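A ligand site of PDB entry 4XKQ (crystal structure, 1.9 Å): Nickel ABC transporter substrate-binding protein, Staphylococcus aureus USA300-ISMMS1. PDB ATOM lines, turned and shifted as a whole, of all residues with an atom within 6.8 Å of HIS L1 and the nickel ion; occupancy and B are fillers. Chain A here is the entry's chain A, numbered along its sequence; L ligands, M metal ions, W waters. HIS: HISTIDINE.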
ATOM      1  N   PRO A  16     -14.993 -24.858 -14.283  1.00  0.00           N
ATOM      2  CA  PRO A  16     -13.538 -24.737 -14.446  1.00  0.00           C
ATOM      3  C   PRO A  16     -13.190 -23.426 -15.195  1.00  0.00           C
ATOM      4  O   PRO A  16     -14.095 -22.733 -15.660  1.00  0.00           O
ATOM      5  CB  PRO A  16     -13.192 -25.956 -15.288  1.00  0.00           C
ATOM      6  CG  PRO A  16     -14.392 -26.061 -16.215  1.00  0.00           C
ATOM      7  CD  PRO A  16     -15.611 -25.608 -15.396  1.00  0.00           C
ATOM      8  N   LEU A  17     -11.893 -23.124 -15.302  1.00  0.00           N
ATOM      9  CA  LEU A  17     -11.322 -22.077 -16.158  1.00  0.00           C
ATOM     10  C   LEU A  17     -11.613 -20.671 -15.620  1.00  0.00           C
ATOM     11  O   LEU A  17     -12.307 -19.861 -16.248  1.00  0.00           O
ATOM     12  CB  LEU A  17     -11.811 -22.228 -17.602  1.00  0.00           C
ATOM     13  CG  LEU A  17     -11.474 -23.632 -18.156  1.00  0.00           C
ATOM     14  CD1 LEU A  17     -11.795 -23.726 -19.655  1.00  0.00           C
ATOM     15  CD2 LEU A  17     -10.023 -24.017 -17.897  1.00  0.00           C
ATOM     16  N   LYS A  18     -11.072 -20.412 -14.435  1.00  0.00           N
ATOM     17  CA  LYS A  18     -11.282 -19.143 -13.763  1.00  0.00           C
ATOM     18  C   LYS A  18     -10.971 -17.963 -14.682  1.00  0.00           C
ATOM     19  O   LYS A  18     -10.064 -18.043 -15.519  1.00  0.00           O
ATOM     20  CB  LYS A  18     -10.424 -19.061 -12.488  1.00  0.00           C
ATOM     21  CG  LYS A  18      -8.933 -19.097 -12.802  1.00  0.00           C
ATOM     22  CD  LYS A  18      -8.083 -18.919 -11.551  1.00  0.00           C
ATOM     23  CE  LYS A  18      -8.086 -20.158 -10.698  1.00  0.00           C
ATOM     24  NZ  LYS A  18      -7.417 -19.916  -9.389  1.00  0.00           N
ATOM     25  N   THR A  19     -11.724 -16.887 -14.522  1.00  0.00           N
ATOM     26  CA  THR A  19     -11.575 -15.685 -15.318  1.00  0.00           C
ATOM     27  C   THR A  19     -10.790 -14.617 -14.552  1.00  0.00           C
ATOM     28  O   THR A  19     -10.642 -14.722 -13.335  1.00  0.00           O
ATOM     29  CB  THR A  19     -12.931 -15.092 -15.676  1.00  0.00           C
ATOM     30  OG1 THR A  19     -13.736 -15.057 -14.484  1.00  0.00           O
ATOM     31  CG2 THR A  19     -13.599 -15.916 -16.771  1.00  0.00           C
ATOM     32  N   THR A  27     -14.635 -13.017 -22.247  1.00  0.00           N
ATOM     33  CA  THR A  27     -14.986 -14.375 -21.828  1.00  0.00           C
ATOM     34  C   THR A  27     -16.438 -14.671 -22.151  1.00  0.00           C
ATOM     35  O   THR A  27     -17.265 -13.766 -22.113  1.00  0.00           O
ATOM     36  CB  THR A  27     -14.765 -14.569 -20.308  1.00  0.00           C
ATOM     37  OG1 THR A  27     -15.343 -15.816 -19.898  1.00  0.00           O
ATOM     38  CG2 THR A  27     -15.407 -13.434 -19.505  1.00  0.00           C
ATOM     39  N   ASP A  28     -16.762 -15.934 -22.448  1.00  0.00           N
ATOM     40  CA  ASP A  28     -18.147 -16.312 -22.710  1.00  0.00           C
ATOM     41  C   ASP A  28     -18.920 -16.621 -21.432  1.00  0.00           C
ATOM     42  O   ASP A  28     -20.122 -16.928 -21.456  1.00  0.00           O
ATOM     43  CB  ASP A  28     -18.191 -17.482 -23.696  1.00  0.00           C
ATOM     44  CG  ASP A  28     -17.641 -18.789 -23.134  1.00  0.00           C
ATOM     45  OD1 ASP A  28     -17.389 -18.915 -21.914  1.00  0.00           O
ATOM     46  OD2 ASP A  28     -17.478 -19.741 -23.955  1.00  0.00           O
ATOM     47  N   ARG A 234     -16.219 -29.711 -29.469  1.00  0.00           N
ATOM     48  CA  ARG A 234     -14.991 -29.323 -28.791  1.00  0.00           C
ATOM     49  C   ARG A 234     -13.906 -30.350 -29.099  1.00  0.00           C
ATOM     50  O   ARG A 234     -14.145 -31.544 -29.097  1.00  0.00           O
ATOM     51  CB  ARG A 234     -15.212 -29.197 -27.289  1.00  0.00           C
ATOM     52  CG  ARG A 234     -13.930 -28.976 -26.498  1.00  0.00           C
ATOM     53  CD  ARG A 234     -14.249 -28.409 -25.135  1.00  0.00           C
ATOM     54  NE  ARG A 234     -14.798 -27.082 -25.285  1.00  0.00           N
ATOM     55  CZ  ARG A 234     -14.052 -25.985 -25.380  1.00  0.00           C
ATOM     56  NH1 ARG A 234     -12.725 -26.054 -25.308  1.00  0.00           N
ATOM     57  NH2 ARG A 234     -14.634 -24.818 -25.528  1.00  0.00           N
ATOM     58  N   TYR A 322      -3.208 -28.158 -17.879  1.00  0.00           N
ATOM     59  CA  TYR A 322      -4.058 -27.485 -16.899  1.00  0.00           C
ATOM     60  C   TYR A 322      -5.197 -28.440 -16.579  1.00  0.00           C
ATOM     61  O   TYR A 322      -5.481 -29.369 -17.358  1.00  0.00           O
ATOM     62  CB  TYR A 322      -4.564 -26.101 -17.409  1.00  0.00           C
ATOM     63  CG  TYR A 322      -5.328 -26.120 -18.727  1.00  0.00           C
ATOM     64  CD1 TYR A 322      -4.658 -26.317 -19.936  1.00  0.00           C
ATOM     65  CD2 TYR A 322      -6.712 -25.940 -18.749  1.00  0.00           C
ATOM     66  CE1 TYR A 322      -5.355 -26.345 -21.156  1.00  0.00           C
ATOM     67  CE2 TYR A 322      -7.422 -25.951 -19.951  1.00  0.00           C
ATOM     68  CZ  TYR A 322      -6.721 -26.163 -21.147  1.00  0.00           C
ATOM     69  OH  TYR A 322      -7.415 -26.199 -22.346  1.00  0.00           O
ATOM     70  N   GLY A 324      -8.549 -27.824 -15.901  1.00  0.00           N
ATOM     71  CA  GLY A 324      -9.924 -27.466 -16.171  1.00  0.00           C
ATOM     72  C   GLY A 324     -10.656 -28.447 -17.076  1.00  0.00           C
ATOM     73  O   GLY A 324     -11.812 -28.792 -16.832  1.00  0.00           O
ATOM     74  N   ARG A 325      -9.977 -28.878 -18.134  1.00  0.00           N
ATOM     75  CA  ARG A 325     -10.488 -29.968 -18.971  1.00  0.00           C
ATOM     76  C   ARG A 325      -9.828 -31.246 -18.408  1.00  0.00           C
ATOM     77  O   ARG A 325      -8.626 -31.445 -18.565  1.00  0.00           O
ATOM     78  CB  ARG A 325     -10.133 -29.749 -20.461  1.00  0.00           C
ATOM     79  CG  ARG A 325     -10.479 -28.356 -21.005  1.00  0.00           C
ATOM     80  CD  ARG A 325     -12.000 -28.186 -21.263  1.00  0.00           C
ATOM     81  NE  ARG A 325     -12.282 -26.816 -21.709  1.00  0.00           N
ATOM     82  CZ  ARG A 325     -13.500 -26.294 -21.828  1.00  0.00           C
ATOM     83  NH1 ARG A 325     -14.570 -27.011 -21.511  1.00  0.00           N
ATOM     84  NH2 ARG A 325     -13.633 -25.043 -22.243  1.00  0.00           N
ATOM     85  N   LEU A 328      -7.078 -33.660 -20.096  1.00  0.00           N
ATOM     86  CA  LEU A 328      -5.894 -33.145 -20.776  1.00  0.00           C
ATOM     87  C   LEU A 328      -4.619 -33.588 -20.080  1.00  0.00           C
ATOM     88  O   LEU A 328      -3.680 -34.025 -20.728  1.00  0.00           O
ATOM     89  CB  LEU A 328      -5.917 -31.612 -20.868  1.00  0.00           C
ATOM     90  CG  LEU A 328      -6.908 -31.035 -21.871  1.00  0.00           C
ATOM     91  CD1 LEU A 328      -6.735 -29.523 -21.922  1.00  0.00           C
ATOM     92  CD2 LEU A 328      -6.743 -31.650 -23.279  1.00  0.00           C
ATOM     93  N   ASP A 353      -3.594 -20.752 -14.628  1.00  0.00           N
ATOM     94  CA  ASP A 353      -4.179 -19.806 -15.572  1.00  0.00           C
ATOM     95  C   ASP A 353      -3.568 -20.055 -16.957  1.00  0.00           C
ATOM     96  O   ASP A 353      -2.556 -19.454 -17.296  1.00  0.00           O
ATOM     97  CB  ASP A 353      -3.929 -18.360 -15.109  1.00  0.00           C
ATOM     98  CG  ASP A 353      -4.317 -17.298 -16.158  1.00  0.00           C
ATOM     99  OD1 ASP A 353      -5.059 -17.604 -17.110  1.00  0.00           O
ATOM    100  OD2 ASP A 353      -3.876 -16.132 -16.006  1.00  0.00           O
ATOM    101  N   ILE A 354      -4.179 -20.942 -17.742  1.00  0.00           N
ATOM    102  CA  ILE A 354      -3.546 -21.327 -18.998  1.00  0.00           C
ATOM    103  C   ILE A 354      -3.433 -20.154 -19.998  1.00  0.00           C
ATOM    104  O   ILE A 354      -2.401 -19.979 -20.640  1.00  0.00           O
ATOM    105  CB  ILE A 354      -4.288 -22.544 -19.653  1.00  0.00           C
ATOM    106  CG1 ILE A 354      -3.522 -23.036 -20.891  1.00  0.00           C
ATOM    107  CG2 ILE A 354      -5.732 -22.191 -20.040  1.00  0.00           C
ATOM    108  CD1 ILE A 354      -2.103 -23.530 -20.611  1.00  0.00           C
ATOM    109  N   GLU A 355      -4.472 -19.342 -20.119  1.00  0.00           N
ATOM    110  CA  GLU A 355      -4.436 -18.274 -21.134  1.00  0.00           C
ATOM    111  C   GLU A 355      -3.341 -17.256 -20.806  1.00  0.00           C
ATOM    112  O   GLU A 355      -2.638 -16.785 -21.686  1.00  0.00           O
ATOM    113  CB  GLU A 355      -5.796 -17.590 -21.244  1.00  0.00           C
ATOM    114  CG  GLU A 355      -6.955 -18.476 -21.744  1.00  0.00           C
ATOM    115  CD  GLU A 355      -6.816 -18.880 -23.213  1.00  0.00           C
ATOM    116  OE1 GLU A 355      -7.331 -18.141 -24.092  1.00  0.00           O
ATOM    117  OE2 GLU A 355      -6.189 -19.925 -23.488  1.00  0.00           O
ATOM    118  N   TYR A 369      -4.340 -28.476 -25.001  1.00  0.00           N
ATOM    119  CA  TYR A 369      -5.313 -27.427 -25.225  1.00  0.00           C
ATOM    120  C   TYR A 369      -6.642 -27.990 -25.686  1.00  0.00           C
ATOM    121  O   TYR A 369      -6.765 -29.160 -25.985  1.00  0.00           O
ATOM    122  CB  TYR A 369      -4.803 -26.425 -26.287  1.00  0.00           C
ATOM    123  CG  TYR A 369      -5.333 -24.997 -26.118  1.00  0.00           C
ATOM    124  CD1 TYR A 369      -4.944 -24.209 -25.031  1.00  0.00           C
ATOM    125  CD2 TYR A 369      -6.204 -24.436 -27.047  1.00  0.00           C
ATOM    126  CE1 TYR A 369      -5.425 -22.882 -24.872  1.00  0.00           C
ATOM    127  CE2 TYR A 369      -6.682 -23.132 -26.897  1.00  0.00           C
ATOM    128  CZ  TYR A 369      -6.283 -22.361 -25.818  1.00  0.00           C
ATOM    129  OH  TYR A 369      -6.762 -21.079 -25.647  1.00  0.00           O
ATOM    130  N   SER A 370      -7.649 -27.127 -25.705  1.00  0.00           N
ATOM    131  CA  SER A 370      -8.993 -27.546 -26.032  1.00  0.00           C
ATOM    132  C   SER A 370      -9.682 -26.348 -26.655  1.00  0.00           C
ATOM    133  O   SER A 370      -9.610 -25.243 -26.117  1.00  0.00           O
ATOM    134  CB  SER A 370      -9.731 -28.010 -24.774  1.00  0.00           C
ATOM    135  OG  SER A 370     -11.086 -28.294 -25.077  1.00  0.00           O
ATOM    136  N   PHE A 371     -10.380 -26.529 -27.769  1.00  0.00           N
ATOM    137  CA  PHE A 371     -11.140 -25.392 -28.226  1.00  0.00           C
ATOM    138  C   PHE A 371     -12.404 -25.799 -28.897  1.00  0.00           C
ATOM    139  O   PHE A 371     -12.557 -26.912 -29.383  1.00  0.00           O
ATOM    140  CB  PHE A 371     -10.332 -24.518 -29.171  1.00  0.00           C
ATOM    141  CG  PHE A 371     -11.022 -23.237 -29.535  1.00  0.00           C
ATOM    142  CD1 PHE A 371     -11.373 -22.308 -28.542  1.00  0.00           C
ATOM    143  CD2 PHE A 371     -11.369 -22.979 -30.840  1.00  0.00           C
ATOM    144  CE1 PHE A 371     -11.984 -21.143 -28.894  1.00  0.00           C
ATOM    145  CE2 PHE A 371     -12.021 -21.825 -31.186  1.00  0.00           C
ATOM    146  CZ  PHE A 371     -12.298 -20.900 -30.205  1.00  0.00           C
ATOM    147  N   GLY A 372     -13.315 -24.844 -28.910  1.00  0.00           N
ATOM    148  CA  GLY A 372     -14.639 -25.044 -29.485  1.00  0.00           C
ATOM    149  C   GLY A 372     -14.465 -24.661 -30.950  1.00  0.00           C
ATOM    150  O   GLY A 372     -14.511 -23.490 -31.283  1.00  0.00           O
ATOM    151  N   ILE A 393      -6.821 -17.007 -30.885  1.00  0.00           N
ATOM    152  CA  ILE A 393      -6.545 -18.278 -30.222  1.00  0.00           C
ATOM    153  C   ILE A 393      -5.314 -18.981 -30.819  1.00  0.00           C
ATOM    154  O   ILE A 393      -5.008 -20.117 -30.491  1.00  0.00           O
ATOM    155  CB  ILE A 393      -7.756 -19.197 -30.284  1.00  0.00           C
ATOM    156  CG1 ILE A 393      -8.071 -19.526 -31.734  1.00  0.00           C
ATOM    157  CG2 ILE A 393      -8.966 -18.521 -29.613  1.00  0.00           C
ATOM    158  CD1 ILE A 393      -9.395 -20.175 -31.919  1.00  0.00           C
ATOM    159  N   LYS A 395      -2.234 -19.321 -30.179  1.00  0.00           N
ATOM    160  CA  LYS A 395      -1.266 -19.123 -29.078  1.00  0.00           C
ATOM    161  C   LYS A 395       0.161 -19.386 -29.540  1.00  0.00           C
ATOM    162  O   LYS A 395       1.108 -18.751 -29.052  1.00  0.00           O
ATOM    163  CB  LYS A 395      -1.601 -20.045 -27.879  1.00  0.00           C
ATOM    164  CG  LYS A 395      -3.041 -20.020 -27.389  1.00  0.00           C
ATOM    165  CD  LYS A 395      -3.495 -18.603 -27.069  1.00  0.00           C
ATOM    166  CE  LYS A 395      -4.898 -18.638 -26.462  1.00  0.00           C
ATOM    167  NZ  LYS A 395      -5.375 -17.268 -26.244  1.00  0.00           N
HETATM  168  N   HIS L   1      -9.463 -22.546 -24.748  1.00  0.00           N
HETATM  169  CA  HIS L   1      -9.017 -23.418 -23.640  1.00  0.00           C
HETATM  170  C   HIS L   1     -10.143 -24.256 -23.042  1.00  0.00           C
HETATM  171  O   HIS L   1     -11.282 -23.864 -23.188  1.00  0.00           O
HETATM  172  CB  HIS L   1      -8.406 -22.600 -22.501  1.00  0.00           C
HETATM  173  CG  HIS L   1      -9.355 -21.635 -21.854  1.00  0.00           C
HETATM  174  ND1 HIS L   1     -10.512 -21.185 -22.467  1.00  0.00           N
HETATM  175  CD2 HIS L   1      -9.313 -21.025 -20.646  1.00  0.00           C
HETATM  176  CE1 HIS L   1     -11.135 -20.340 -21.660  1.00  0.00           C
HETATM  177  NE2 HIS L   1     -10.432 -20.226 -20.554  1.00  0.00           N
HETATM  178  OXT HIS L   1      -9.944 -25.317 -22.396  1.00  0.00           O
HETATM  179  N   HIS L   2     -13.141 -21.385 -23.583  1.00  0.00           N
HETATM  180  CA  HIS L   2     -13.881 -21.337 -24.830  1.00  0.00           C
HETATM  181  C   HIS L   2     -13.281 -22.332 -25.835  1.00  0.00           C
HETATM  182  O   HIS L   2     -13.975 -22.760 -26.777  1.00  0.00           O
HETATM  183  CB  HIS L   2     -13.850 -19.926 -25.405  1.00  0.00           C
HETATM  184  CG  HIS L   2     -12.475 -19.450 -25.731  1.00  0.00           C
HETATM  185  ND1 HIS L   2     -11.335 -20.087 -25.264  1.00  0.00           N
HETATM  186  CD2 HIS L   2     -12.042 -18.402 -26.471  1.00  0.00           C
HETATM  187  CE1 HIS L   2     -10.266 -19.451 -25.699  1.00  0.00           C
HETATM  188  NE2 HIS L   2     -10.667 -18.411 -26.426  1.00  0.00           N
HETATM  189  OXT HIS L   2     -12.099 -22.736 -25.714  1.00  0.00           O
HETATM  190 NI    NI M   1     -11.246 -21.955 -24.145  1.00  0.00          NI
HETATM  191  O   HOH W   1     -11.390 -18.379 -18.473  1.00  0.00           O
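No residue comes within 4 Å of the nickel ion.
Residues that only touch HIS L1: Leu 17, Ile 354 and Glu 355. Hydrophobic or aromatic side chains that line HIS L1: Leu 17, Tyr 322, Ile 354 and Tyr 369. Within 4 Å of HIS L1: Leu 17, Arg 234, Tyr 322, Arg 325, Ile 354, Glu 355, Tyr 369 and Ser 370.
The nickel ion is bound by OXT of HIS L2 (1.9 Å), N of HIS L1 (2.0 Å), ND1 of HIS L1 (2.0 Å), N of HIS L2 (2.1 Å), O of HIS L1 (2.1 Å) and ND1 of HIS L2 (2.2 Å).
Water W1 lies within hydrogen-bond range of the backbone carbonyl oxygen (O) of Leu 17 (2.8 Å), a nitrogen (NE2) of HIS L1 (2.9 Å) and the backbone carbonyl oxygen (O) of Lys 18 (3.3 Å).
The guanidinium group of Arg 234 lies within salt-bridge range of an oxygen (O) of HIS L2 (2.5 Å). An oxygen (OXT) of HIS L1 lies within salt-bridge range of the guanidinium group of Arg 325, 2.9 Å away. A nitrogen (N) of HIS L1 sits close to the side-chain hydroxyl of Tyr 369 (3.2 Å). N of Gly 372 is in hydrogen-bond range of O of HIS L2 (3.1 Å). O of Ser 370 lies close to N of HIS L1 (3.0 Å). An oxygen (OXT) of HIS L1 lies within hydrogen-bond range of the side-chain hydroxyl (OH) of Tyr 322, 2.7 Å away. The guanidinium group (NH1) of Arg 234 lies close to an oxygen (O) of HIS L1, at 3.4 Å.
The side-chain amino group (NZ) of Lys 395 lies within salt-bridge range of the side-chain carboxylate (OE1) of Glu 355, 3.0 Å away. The side-chain hydroxyl (OH) of Tyr 322 is in hydrogen-bond range of the backbone NH (N) of Ser 370 (3.5 Å). OH of Tyr 369 sits at hydrogen-bond distance from OE2 of Glu 355 (2.5 Å). NH1 of Arg 234 sits at hydrogen-bond distance from OG of Ser 370, 2.8 Å away.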
